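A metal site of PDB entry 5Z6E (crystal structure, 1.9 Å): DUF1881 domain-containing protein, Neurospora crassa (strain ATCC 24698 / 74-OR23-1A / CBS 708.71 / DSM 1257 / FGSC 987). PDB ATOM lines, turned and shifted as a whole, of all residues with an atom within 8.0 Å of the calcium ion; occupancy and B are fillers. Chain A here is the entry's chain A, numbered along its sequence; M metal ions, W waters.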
ATOM      1  N   VAL A  33     -18.004 -30.019  -9.133  1.00  0.00           N
ATOM      2  CA  VAL A  33     -19.171 -29.793  -9.971  1.00  0.00           C
ATOM      3  C   VAL A  33     -18.926 -28.587 -10.896  1.00  0.00           C
ATOM      4  O   VAL A  33     -18.420 -27.570 -10.454  1.00  0.00           O
ATOM      5  CB  VAL A  33     -20.408 -29.564  -9.085  1.00  0.00           C
ATOM      6  CG1 VAL A  33     -21.635 -29.271  -9.918  1.00  0.00           C
ATOM      7  CG2 VAL A  33     -20.636 -30.805  -8.202  1.00  0.00           C
ATOM      8  N   ASN A  38     -23.201 -25.872 -10.263  1.00  0.00           N
ATOM      9  CA  ASN A  38     -22.841 -25.716  -8.858  1.00  0.00           C
ATOM     10  C   ASN A  38     -24.072 -25.471  -7.985  1.00  0.00           C
ATOM     11  O   ASN A  38     -24.892 -24.626  -8.302  1.00  0.00           O
ATOM     12  CB  ASN A  38     -21.847 -24.568  -8.701  1.00  0.00           C
ATOM     13  CG  ASN A  38     -21.279 -24.489  -7.315  1.00  0.00           C
ATOM     14  OD1 ASN A  38     -21.137 -23.401  -6.729  1.00  0.00           O
ATOM     15  ND2 ASN A  38     -20.953 -25.649  -6.766  1.00  0.00           N
ATOM     16  N   ASP A  39     -24.163 -26.239  -6.892  1.00  0.00           N
ATOM     17  CA  ASP A  39     -25.290 -26.247  -5.945  1.00  0.00           C
ATOM     18  C   ASP A  39     -26.644 -26.666  -6.556  1.00  0.00           C
ATOM     19  O   ASP A  39     -27.673 -26.556  -5.885  1.00  0.00           O
ATOM     20  CB  ASP A  39     -25.469 -24.863  -5.297  1.00  0.00           C
ATOM     21  CG  ASP A  39     -24.233 -24.390  -4.562  1.00  0.00           C
ATOM     22  OD1 ASP A  39     -23.385 -25.222  -4.140  1.00  0.00           O
ATOM     23  OD2 ASP A  39     -24.093 -23.152  -4.425  1.00  0.00           O
ATOM     24  N   LYS A  40     -26.638 -27.152  -7.800  1.00  0.00           N
ATOM     25  CA  LYS A  40     -27.902 -27.427  -8.477  1.00  0.00           C
ATOM     26  C   LYS A  40     -28.407 -28.864  -8.331  1.00  0.00           C
ATOM     27  O   LYS A  40     -29.517 -29.160  -8.760  1.00  0.00           O
ATOM     28  CB  LYS A  40     -27.797 -27.142  -9.990  1.00  0.00           C
ATOM     29  CG  LYS A  40     -27.363 -25.737 -10.375  1.00  0.00           C
ATOM     30  CD  LYS A  40     -28.269 -24.665  -9.865  1.00  0.00           C
ATOM     31  CE  LYS A  40     -27.879 -23.322 -10.479  1.00  0.00           C
ATOM     32  NZ  LYS A  40     -28.470 -22.174  -9.733  1.00  0.00           N
ATOM     33  N   TRP A  55     -19.231 -32.782  -0.257  1.00  0.00           N
ATOM     34  CA  TRP A  55     -18.995 -31.545   0.476  1.00  0.00           C
ATOM     35  C   TRP A  55     -19.767 -30.352  -0.089  1.00  0.00           C
ATOM     36  O   TRP A  55     -19.952 -30.214  -1.311  1.00  0.00           O
ATOM     37  CB  TRP A  55     -17.512 -31.158   0.485  1.00  0.00           C
ATOM     38  CG  TRP A  55     -16.556 -32.136   1.087  1.00  0.00           C
ATOM     39  CD1 TRP A  55     -16.084 -32.148   2.375  1.00  0.00           C
ATOM     40  CD2 TRP A  55     -15.908 -33.220   0.414  1.00  0.00           C
ATOM     41  NE1 TRP A  55     -15.190 -33.184   2.531  1.00  0.00           N
ATOM     42  CE2 TRP A  55     -15.071 -33.855   1.346  1.00  0.00           C
ATOM     43  CE3 TRP A  55     -15.969 -33.713  -0.890  1.00  0.00           C
ATOM     44  CZ2 TRP A  55     -14.292 -34.961   1.013  1.00  0.00           C
ATOM     45  CZ3 TRP A  55     -15.191 -34.818  -1.224  1.00  0.00           C
ATOM     46  CH2 TRP A  55     -14.373 -35.427  -0.276  1.00  0.00           C
ATOM     47  N   GLN A  56     -20.152 -29.476   0.819  1.00  0.00           N
ATOM     48  CA  GLN A  56     -20.693 -28.175   0.485  1.00  0.00           C
ATOM     49  C   GLN A  56     -19.746 -27.306  -0.360  1.00  0.00           C
ATOM     50  O   GLN A  56     -20.160 -26.676  -1.321  1.00  0.00           O
ATOM     51  CB  GLN A  56     -21.059 -27.440   1.771  1.00  0.00           C
ATOM     52  CG  GLN A  56     -21.689 -26.085   1.561  1.00  0.00           C
ATOM     53  CD  GLN A  56     -22.036 -25.416   2.874  1.00  0.00           C
ATOM     54  OE1 GLN A  56     -21.547 -25.808   3.932  1.00  0.00           O
ATOM     55  NE2 GLN A  56     -22.890 -24.392   2.815  1.00  0.00           N
ATOM     56  N   HIS A  57     -18.462 -27.277   0.016  1.00  0.00           N
ATOM     57  CA  HIS A  57     -17.505 -26.390  -0.641  1.00  0.00           C
ATOM     58  C   HIS A  57     -16.507 -27.145  -1.490  1.00  0.00           C
ATOM     59  O   HIS A  57     -16.134 -28.273  -1.163  1.00  0.00           O
ATOM     60  CB  HIS A  57     -16.737 -25.560   0.392  1.00  0.00           C
ATOM     61  CG  HIS A  57     -17.607 -24.731   1.290  1.00  0.00           C
ATOM     62  ND1 HIS A  57     -18.736 -24.076   0.841  1.00  0.00           N
ATOM     63  CD2 HIS A  57     -17.506 -24.437   2.603  1.00  0.00           C
ATOM     64  CE1 HIS A  57     -19.292 -23.417   1.837  1.00  0.00           C
ATOM     65  NE2 HIS A  57     -18.565 -23.630   2.925  1.00  0.00           N
ATOM     66  N   TYR A  58     -16.061 -26.503  -2.576  1.00  0.00           N
ATOM     67  CA  TYR A  58     -15.086 -27.075  -3.512  1.00  0.00           C
ATOM     68  C   TYR A  58     -13.802 -27.558  -2.868  1.00  0.00           C
ATOM     69  O   TYR A  58     -13.172 -28.492  -3.373  1.00  0.00           O
ATOM     70  CB  TYR A  58     -14.723 -26.034  -4.578  1.00  0.00           C
ATOM     71  CG  TYR A  58     -15.698 -25.901  -5.712  1.00  0.00           C
ATOM     72  CD1 TYR A  58     -16.007 -26.983  -6.527  1.00  0.00           C
ATOM     73  CD2 TYR A  58     -16.283 -24.674  -5.989  1.00  0.00           C
ATOM     74  CE1 TYR A  58     -16.900 -26.849  -7.585  1.00  0.00           C
ATOM     75  CE2 TYR A  58     -17.167 -24.534  -7.028  1.00  0.00           C
ATOM     76  CZ  TYR A  58     -17.469 -25.624  -7.833  1.00  0.00           C
ATOM     77  OH  TYR A  58     -18.345 -25.463  -8.872  1.00  0.00           O
ATOM     78  N   THR A  61     -14.613 -28.671   2.377  1.00  0.00           N
ATOM     79  CA  THR A  61     -15.011 -28.159   3.685  1.00  0.00           C
ATOM     80  C   THR A  61     -16.514 -27.874   3.671  1.00  0.00           C
ATOM     81  O   THR A  61     -17.196 -28.070   2.658  1.00  0.00           O
ATOM     82  CB  THR A  61     -14.246 -26.888   4.064  1.00  0.00           C
ATOM     83  OG1 THR A  61     -14.578 -25.848   3.144  1.00  0.00           O
ATOM     84  CG2 THR A  61     -12.731 -27.149   4.025  1.00  0.00           C
ATOM     85  N   ILE A  77     -27.170 -30.331   2.574  1.00  0.00           N
ATOM     86  CA  ILE A  77     -25.716 -30.114   2.476  1.00  0.00           C
ATOM     87  C   ILE A  77     -25.461 -28.638   2.126  1.00  0.00           C
ATOM     88  O   ILE A  77     -24.328 -28.155   2.129  1.00  0.00           O
ATOM     89  CB  ILE A  77     -25.037 -31.062   1.444  1.00  0.00           C
ATOM     90  CG1 ILE A  77     -23.554 -31.256   1.802  1.00  0.00           C
ATOM     91  CG2 ILE A  77     -25.249 -30.579   0.017  1.00  0.00           C
ATOM     92  CD1 ILE A  77     -22.821 -32.290   0.935  1.00  0.00           C
ATOM     93  N   GLY A  78     -26.542 -27.907   1.850  1.00  0.00           N
ATOM     94  CA  GLY A  78     -26.456 -26.462   1.678  1.00  0.00           C
ATOM     95  C   GLY A  78     -25.775 -26.008   0.398  1.00  0.00           C
ATOM     96  O   GLY A  78     -25.137 -24.953   0.357  1.00  0.00           O
ATOM     97  N   GLY A  79     -25.926 -26.815  -0.650  1.00  0.00           N
ATOM     98  CA  GLY A  79     -25.369 -26.513  -1.962  1.00  0.00           C
ATOM     99  C   GLY A  79     -24.186 -27.395  -2.270  1.00  0.00           C
ATOM    100  O   GLY A  79     -23.049 -27.095  -1.859  1.00  0.00           O
ATOM    101  N   LEU A  80     -24.428 -28.485  -3.005  1.00  0.00           N
ATOM    102  CA  LEU A  80     -23.379 -29.458  -3.319  1.00  0.00           C
ATOM    103  C   LEU A  80     -22.382 -28.930  -4.333  1.00  0.00           C
ATOM    104  O   LEU A  80     -22.767 -28.555  -5.430  1.00  0.00           O
ATOM    105  CB  LEU A  80     -24.003 -30.755  -3.826  1.00  0.00           C
ATOM    106  CG  LEU A  80     -23.026 -31.812  -4.346  1.00  0.00           C
ATOM    107  CD1 LEU A  80     -22.095 -32.227  -3.208  1.00  0.00           C
ATOM    108  CD2 LEU A  80     -23.805 -33.003  -4.936  1.00  0.00           C
ATOM    109  N   SER A  81     -21.092 -28.907  -3.978  1.00  0.00           N
ATOM    110  CA  SER A  81     -20.073 -28.428  -4.911  1.00  0.00           C
ATOM    111  C   SER A  81     -19.000 -29.448  -5.271  1.00  0.00           C
ATOM    112  O   SER A  81     -18.361 -29.336  -6.312  1.00  0.00           O
ATOM    113  CB  SER A  81     -19.392 -27.179  -4.348  1.00  0.00           C
ATOM    114  OG  SER A  81     -20.307 -26.088  -4.305  1.00  0.00           O
ATOM    115  N   ARG A  82     -18.775 -30.431  -4.414  1.00  0.00           N
ATOM    116  CA  ARG A  82     -17.739 -31.423  -4.691  1.00  0.00           C
ATOM    117  C   ARG A  82     -18.110 -32.768  -4.114  1.00  0.00           C
ATOM    118  O   ARG A  82     -18.695 -32.849  -3.034  1.00  0.00           O
ATOM    119  CB  ARG A  82     -16.400 -30.960  -4.138  1.00  0.00           C
ATOM    120  CG  ARG A  82     -15.303 -31.991  -4.302  1.00  0.00           C
ATOM    121  CD  ARG A  82     -13.957 -31.371  -4.307  1.00  0.00           C
ATOM    122  NE  ARG A  82     -12.901 -32.383  -4.318  1.00  0.00           N
ATOM    123  CZ  ARG A  82     -12.318 -32.845  -5.417  1.00  0.00           C
ATOM    124  NH1 ARG A  82     -12.681 -32.381  -6.597  1.00  0.00           N
ATOM    125  NH2 ARG A  82     -11.364 -33.764  -5.317  1.00  0.00           N
HETATM  126 CA    CA M   1     -21.581 -25.194  -2.536  1.00  0.00          CA
HETATM  127  O   HOH W   1     -22.820 -24.018  -0.934  1.00  0.00           O
HETATM  128  O   HOH W   2     -21.495 -23.112  -3.893  1.00  0.00           O
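Water W2 bridges OD2 of Asp 39 (2.7 Å) and OD1 of Asn 38 (2.9 Å).
The side-chain hydroxyl of Ser 81 lies close to the side-chain amide nitrogen of Asn 38, at 2.6 Å. O of Trp 55 sits at hydrogen-bond distance from N of Ser 81 (3.2 Å). N of Val 33 is in hydrogen-bond range of O of Ser 81 (2.9 Å). The side-chain amide nitrogen (NE2) of Gln 56 sits at hydrogen-bond distance from the backbone carbonyl oxygen (O) of Gly 78 (3.4 Å). N of Asp 39 sits at hydrogen-bond distance from O of Leu 80 (3.1 Å).
The calcium ion is bound by water W1 (2.3 Å), OG of Ser 81 (2.4 Å), O of Gln 56 (2.4 Å), OD1 of Asp 39 (2.4 Å), water W2 (2.5 Å) and O of Gly 79 (2.5 Å).
Four residues have an atom within 4 Å of the calcium ion: Asp 39, Gln 56, Gly 79 and Ser 81. Along chain A the residues within 4 Å of the calcium ion span positions 39 to 81. The nearest printed residue that does not touch the calcium ion is Leu 80 (4.2 Å).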
